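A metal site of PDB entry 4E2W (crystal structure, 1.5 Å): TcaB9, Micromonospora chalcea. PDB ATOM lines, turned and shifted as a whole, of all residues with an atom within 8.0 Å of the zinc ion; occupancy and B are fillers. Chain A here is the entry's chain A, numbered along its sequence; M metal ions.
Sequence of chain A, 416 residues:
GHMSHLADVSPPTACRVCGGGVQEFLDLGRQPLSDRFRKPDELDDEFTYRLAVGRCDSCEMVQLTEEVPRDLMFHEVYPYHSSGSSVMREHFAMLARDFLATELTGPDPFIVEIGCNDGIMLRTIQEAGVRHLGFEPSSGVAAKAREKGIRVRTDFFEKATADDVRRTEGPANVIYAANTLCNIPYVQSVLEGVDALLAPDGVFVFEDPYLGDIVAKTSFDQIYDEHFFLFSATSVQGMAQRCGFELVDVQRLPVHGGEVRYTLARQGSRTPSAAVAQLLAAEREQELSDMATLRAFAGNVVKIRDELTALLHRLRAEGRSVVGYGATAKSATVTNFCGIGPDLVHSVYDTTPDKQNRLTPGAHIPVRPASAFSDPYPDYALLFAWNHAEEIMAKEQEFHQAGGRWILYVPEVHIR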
ATOM      1  N   ALA A  14       0.248 -27.583  12.996  1.00  0.00           N
ATOM      2  CA  ALA A  14      -0.771 -28.174  13.865  1.00  0.00           C
ATOM      3  C   ALA A  14      -2.162 -27.625  13.483  1.00  0.00           C
ATOM      4  O   ALA A  14      -2.332 -26.413  13.319  1.00  0.00           O
ATOM      5  CB  ALA A  14      -0.454 -27.806  15.313  1.00  0.00           C
ATOM      6  N   CYS A  15      -3.162 -28.494  13.342  1.00  0.00           N
ATOM      7  CA  CYS A  15      -4.556 -28.076  13.176  1.00  0.00           C
ATOM      8  C   CYS A  15      -4.996 -27.060  14.238  1.00  0.00           C
ATOM      9  O   CYS A  15      -4.836 -27.306  15.441  1.00  0.00           O
ATOM     10  CB  CYS A  15      -5.484 -29.292  13.148  1.00  0.00           C
ATOM     11  SG  CYS A  15      -7.259 -28.942  12.979  1.00  0.00           S
ATOM     12  N   ARG A  16      -5.560 -25.937  13.808  1.00  0.00           N
ATOM     13  CA  ARG A  16      -6.121 -24.905  14.670  1.00  0.00           C
ATOM     14  C   ARG A  16      -7.408 -25.325  15.367  1.00  0.00           C
ATOM     15  O   ARG A  16      -7.829 -24.661  16.323  1.00  0.00           O
ATOM     16  CB  ARG A  16      -6.323 -23.613  13.859  1.00  0.00           C
ATOM     17  CG  ARG A  16      -4.983 -22.913  13.680  1.00  0.00           C
ATOM     18  CD  ARG A  16      -4.468 -22.455  15.078  1.00  0.00           C
ATOM     19  NE  ARG A  16      -4.214 -21.013  15.099  1.00  0.00           N
ATOM     20  CZ  ARG A  16      -4.566 -20.135  16.040  1.00  0.00           C
ATOM     21  NH1 ARG A  16      -4.233 -18.871  15.864  1.00  0.00           N
ATOM     22  NH2 ARG A  16      -5.234 -20.474  17.143  1.00  0.00           N
ATOM     23  N   VAL A  17      -8.012 -26.429  14.909  1.00  0.00           N
ATOM     24  CA  VAL A  17      -9.192 -26.918  15.633  1.00  0.00           C
ATOM     25  C   VAL A  17      -8.843 -27.930  16.727  1.00  0.00           C
ATOM     26  O   VAL A  17      -9.318 -27.817  17.855  1.00  0.00           O
ATOM     27  CB  VAL A  17     -10.262 -27.545  14.689  1.00  0.00           C
ATOM     28  CG1 VAL A  17     -11.400 -28.082  15.523  1.00  0.00           C
ATOM     29  CG2 VAL A  17     -10.845 -26.454  13.794  1.00  0.00           C
ATOM     30  N   CYS A  18      -8.012 -28.933  16.410  1.00  0.00           N
ATOM     31  CA  CYS A  18      -7.879 -30.072  17.319  1.00  0.00           C
ATOM     32  C   CYS A  18      -6.415 -30.377  17.611  1.00  0.00           C
ATOM     33  O   CYS A  18      -6.127 -31.268  18.400  1.00  0.00           O
ATOM     34  CB  CYS A  18      -8.592 -31.326  16.783  1.00  0.00           C
ATOM     35  SG  CYS A  18      -7.629 -32.113  15.441  1.00  0.00           S
ATOM     36  N   GLY A  19      -5.480 -29.680  16.972  1.00  0.00           N
ATOM     37  CA  GLY A  19      -4.055 -29.959  17.180  1.00  0.00           C
ATOM     38  C   GLY A  19      -3.496 -31.155  16.420  1.00  0.00           C
ATOM     39  O   GLY A  19      -2.300 -31.440  16.566  1.00  0.00           O
ATOM     40  N   GLY A  20      -4.327 -31.824  15.615  1.00  0.00           N
ATOM     41  CA  GLY A  20      -3.883 -32.893  14.732  1.00  0.00           C
ATOM     42  C   GLY A  20      -2.814 -32.440  13.740  1.00  0.00           C
ATOM     43  O   GLY A  20      -2.538 -31.250  13.594  1.00  0.00           O
ATOM     44  N   GLY A  21      -2.260 -33.401  13.014  1.00  0.00           N
ATOM     45  CA  GLY A  21      -1.384 -33.061  11.896  1.00  0.00           C
ATOM     46  C   GLY A  21      -2.110 -32.660  10.619  1.00  0.00           C
ATOM     47  O   GLY A  21      -3.058 -33.340  10.193  1.00  0.00           O
ATOM     48  N   VAL A  22      -1.655 -31.572  10.001  1.00  0.00           N
ATOM     49  CA  VAL A  22      -2.201 -31.106   8.714  1.00  0.00           C
ATOM     50  C   VAL A  22      -1.329 -31.486   7.531  1.00  0.00           C
ATOM     51  O   VAL A  22      -0.154 -31.135   7.513  1.00  0.00           O
ATOM     52  CB  VAL A  22      -2.323 -29.567   8.694  1.00  0.00           C
ATOM     53  CG1 VAL A  22      -2.785 -28.950   7.380  1.00  0.00           C
ATOM     54  CG2 VAL A  22      -3.305 -29.164   9.815  1.00  0.00           C
ATOM     55  N   ARG A  55      -5.095 -30.579   5.015  1.00  0.00           N
ATOM     56  CA  ARG A  55      -6.248 -31.203   5.669  1.00  0.00           C
ATOM     57  C   ARG A  55      -5.755 -31.823   6.965  1.00  0.00           C
ATOM     58  O   ARG A  55      -4.742 -32.539   6.957  1.00  0.00           O
ATOM     59  CB  ARG A  55      -6.981 -32.237   4.769  1.00  0.00           C
ATOM     60  CG  ARG A  55      -8.268 -32.730   5.418  1.00  0.00           C
ATOM     61  CD  ARG A  55      -8.618 -34.179   5.059  1.00  0.00           C
ATOM     62  NE  ARG A  55      -7.729 -35.111   5.736  1.00  0.00           N
ATOM     63  CZ  ARG A  55      -7.681 -36.418   5.501  1.00  0.00           C
ATOM     64  NH1 ARG A  55      -6.821 -37.172   6.168  1.00  0.00           N
ATOM     65  NH2 ARG A  55      -8.477 -36.962   4.583  1.00  0.00           N
ATOM     66  N   CYS A  56      -6.465 -31.593   8.068  1.00  0.00           N
ATOM     67  CA  CYS A  56      -6.113 -32.182   9.356  1.00  0.00           C
ATOM     68  C   CYS A  56      -6.319 -33.697   9.280  1.00  0.00           C
ATOM     69  O   CYS A  56      -7.345 -34.149   8.751  1.00  0.00           O
ATOM     70  CB  CYS A  56      -7.007 -31.633  10.477  1.00  0.00           C
ATOM     71  SG  CYS A  56      -6.550 -32.510  12.007  1.00  0.00           S
ATOM     72  N   ASP A  57      -5.363 -34.464   9.812  1.00  0.00           N
ATOM     73  CA  ASP A  57      -5.463 -35.927   9.877  1.00  0.00           C
ATOM     74  C   ASP A  57      -6.517 -36.491  10.834  1.00  0.00           C
ATOM     75  O   ASP A  57      -6.910 -37.653  10.717  1.00  0.00           O
ATOM     76  CB  ASP A  57      -4.214 -36.539  10.524  1.00  0.00           C
ATOM     77  CG  ASP A  57      -3.012 -36.485   9.637  1.00  0.00           C
ATOM     78  OD1 ASP A  57      -3.250 -36.381   8.411  1.00  0.00           O
ATOM     79  OD2 ASP A  57      -1.910 -36.535  10.223  1.00  0.00           O
ATOM     80  N   SER A  58      -6.963 -35.679  11.781  1.00  0.00           N
ATOM     81  CA  SER A  58      -7.738 -36.194  12.887  1.00  0.00           C
ATOM     82  C   SER A  58      -9.175 -35.720  12.744  1.00  0.00           C
ATOM     83  O   SER A  58     -10.093 -36.513  12.945  1.00  0.00           O
ATOM     84  CB  SER A  58      -7.170 -35.625  14.182  1.00  0.00           C
ATOM     85  OG  SER A  58      -5.982 -36.336  14.487  1.00  0.00           O
ATOM     86  N   CYS A  59      -9.388 -34.447  12.422  1.00  0.00           N
ATOM     87  CA  CYS A  59     -10.749 -33.937  12.341  1.00  0.00           C
ATOM     88  C   CYS A  59     -11.246 -33.574  10.937  1.00  0.00           C
ATOM     89  O   CYS A  59     -12.401 -33.151  10.774  1.00  0.00           O
ATOM     90  CB  CYS A  59     -10.911 -32.725  13.274  1.00  0.00           C
ATOM     91  SG  CYS A  59     -10.201 -31.230  12.494  1.00  0.00           S
ATOM     92  N   GLU A  60     -10.400 -33.726   9.926  1.00  0.00           N
ATOM     93  CA  GLU A  60     -10.791 -33.498   8.522  1.00  0.00           C
ATOM     94  C   GLU A  60     -10.958 -32.047   8.089  1.00  0.00           C
ATOM     95  O   GLU A  60     -11.337 -31.765   6.953  1.00  0.00           O
ATOM     96  CB  GLU A  60     -11.886 -34.390   7.933  1.00  0.00           C
ATOM     97  CG  GLU A  60     -11.459 -35.853   8.191  1.00  0.00           C
ATOM     98  CD  GLU A  60     -12.551 -36.750   7.629  1.00  0.00           C
ATOM     99  OE1 GLU A  60     -12.532 -36.879   6.392  1.00  0.00           O
ATOM    100  OE2 GLU A  60     -13.425 -37.266   8.371  1.00  0.00           O
ATOM    101  N   MET A  61     -10.608 -31.143   8.997  1.00  0.00           N
ATOM    102  CA  MET A  61     -10.649 -29.715   8.696  1.00  0.00           C
ATOM    103  C   MET A  61      -9.611 -29.305   7.643  1.00  0.00           C
ATOM    104  O   MET A  61      -8.389 -29.439   7.826  1.00  0.00           O
ATOM    105  CB  MET A  61     -10.389 -28.900   9.960  1.00  0.00           C
ATOM    106  CG  MET A  61     -10.637 -27.424   9.685  1.00  0.00           C
ATOM    107  SD  MET A  61     -12.283 -26.873   9.160  1.00  0.00           S
ATOM    108  CE  MET A  61     -13.260 -26.949  10.653  1.00  0.00           C
ATOM    109  N   VAL A  62     -10.098 -28.723   6.542  1.00  0.00           N
ATOM    110  CA  VAL A  62      -9.188 -28.214   5.499  1.00  0.00           C
ATOM    111  C   VAL A  62      -8.884 -26.759   5.857  1.00  0.00           C
ATOM    112  O   VAL A  62      -9.774 -25.983   6.164  1.00  0.00           O
ATOM    113  CB  VAL A  62      -9.957 -28.273   4.170  1.00  0.00           C
ATOM    114  CG1 VAL A  62      -9.240 -27.465   3.056  1.00  0.00           C
ATOM    115  CG2 VAL A  62     -10.191 -29.757   3.879  1.00  0.00           C
ATOM    116  N   GLN A  63      -7.614 -26.362   5.843  1.00  0.00           N
ATOM    117  CA  GLN A  63      -7.172 -25.062   6.354  1.00  0.00           C
ATOM    118  C   GLN A  63      -5.836 -24.648   5.722  1.00  0.00           C
ATOM    119  O   GLN A  63      -5.074 -25.512   5.284  1.00  0.00           O
ATOM    120  CB  GLN A  63      -6.981 -25.080   7.866  1.00  0.00           C
ATOM    121  CG  GLN A  63      -5.880 -26.032   8.349  1.00  0.00           C
ATOM    122  CD  GLN A  63      -6.180 -26.508   9.740  1.00  0.00           C
ATOM    123  OE1 GLN A  63      -5.720 -25.877  10.704  1.00  0.00           O
ATOM    124  NE2 GLN A  63      -6.962 -27.581   9.863  1.00  0.00           N
ATOM    125  N   PHE A 229     -10.159 -21.326   6.642  1.00  0.00           N
ATOM    126  CA  PHE A 229     -10.812 -22.635   6.638  1.00  0.00           C
ATOM    127  C   PHE A 229     -11.699 -22.758   5.412  1.00  0.00           C
ATOM    128  O   PHE A 229     -12.369 -21.796   5.004  1.00  0.00           O
ATOM    129  CB  PHE A 229     -11.776 -22.755   7.840  1.00  0.00           C
ATOM    130  CG  PHE A 229     -11.020 -22.815   9.143  1.00  0.00           C
ATOM    131  CD1 PHE A 229     -10.161 -23.897   9.394  1.00  0.00           C
ATOM    132  CD2 PHE A 229     -11.088 -21.791  10.077  1.00  0.00           C
ATOM    133  CE1 PHE A 229      -9.433 -23.946  10.601  1.00  0.00           C
ATOM    134  CE2 PHE A 229     -10.383 -21.814  11.269  1.00  0.00           C
ATOM    135  CZ  PHE A 229      -9.564 -22.931  11.555  1.00  0.00           C
ATOM    136  N   SER A 235     -16.290 -31.653   8.849  1.00  0.00           N
ATOM    137  CA  SER A 235     -15.397 -30.934   9.772  1.00  0.00           C
ATOM    138  C   SER A 235     -16.087 -30.033  10.784  1.00  0.00           C
ATOM    139  O   SER A 235     -15.628 -29.878  11.935  1.00  0.00           O
ATOM    140  CB  SER A 235     -14.291 -30.260   8.929  1.00  0.00           C
ATOM    141  OG  SER A 235     -14.778 -29.111   8.271  1.00  0.00           O
ATOM    142  N   MET A 239     -15.800 -30.107  14.796  1.00  0.00           N
ATOM    143  CA  MET A 239     -15.431 -28.924  15.547  1.00  0.00           C
ATOM    144  C   MET A 239     -16.476 -28.558  16.611  1.00  0.00           C
ATOM    145  O   MET A 239     -16.154 -28.166  17.745  1.00  0.00           O
ATOM    146  CB  MET A 239     -15.269 -27.784  14.524  1.00  0.00           C
ATOM    147  CG  MET A 239     -14.995 -26.410  15.153  1.00  0.00           C
ATOM    148  SD  MET A 239     -14.763 -25.084  13.930  1.00  0.00           S
ATOM    149  CE  MET A 239     -16.442 -24.802  13.363  1.00  0.00           C
ATOM    150  N   ARG A 242     -16.441 -31.205  19.534  1.00  0.00           N
ATOM    151  CA  ARG A 242     -15.292 -31.106  20.415  1.00  0.00           C
ATOM    152  C   ARG A 242     -15.460 -29.965  21.423  1.00  0.00           C
ATOM    153  O   ARG A 242     -14.815 -29.967  22.453  1.00  0.00           O
ATOM    154  CB  ARG A 242     -14.010 -30.992  19.586  1.00  0.00           C
ATOM    155  CG  ARG A 242     -13.625 -32.254  18.807  1.00  0.00           C
ATOM    156  CD  ARG A 242     -12.460 -31.891  17.861  1.00  0.00           C
ATOM    157  NE  ARG A 242     -11.661 -33.048  17.485  1.00  0.00           N
ATOM    158  CZ  ARG A 242     -11.972 -33.915  16.529  1.00  0.00           C
ATOM    159  NH1 ARG A 242     -13.087 -33.766  15.809  1.00  0.00           N
ATOM    160  NH2 ARG A 242     -11.131 -34.914  16.297  1.00  0.00           N
HETATM  161 ZN    ZN M   1      -8.032 -31.130  13.352  1.00  0.00          ZN
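The side-chain sulfur (SG) of Cys 59 lies close to the backbone NH (N) of Met 61.
The backbone NH (N) of Cys 56 is in hydrogen-bond range of the backbone carbonyl oxygen (O) of Met 61.
The backbone NH of Cys 15 is in hydrogen-bond range of the backbone carbonyl oxygen of Gly 20, 2.8 Å away.
The side-chain sulfur of Cys 56 sits close to the backbone NH of Ser 58 (3.2 Å).
SG of Cys 18 lies close to N of Gly 20.
The side-chain sulfur of Cys 15 lies close to the backbone NH of Val 17, at 3.3 Å.
The side-chain amide nitrogen (NE2) of Gln 63 lies close to the side-chain sulfur (SG) of Cys 15, 3.4 Å away.
The zinc ion is bound by SG of Cys 59 (2.3 Å), SG of Cys 18 (2.3 Å), SG of Cys 15 (2.4 Å) and SG of Cys 56 (2.4 Å).
The zinc ion has four donor atoms within binding distance.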
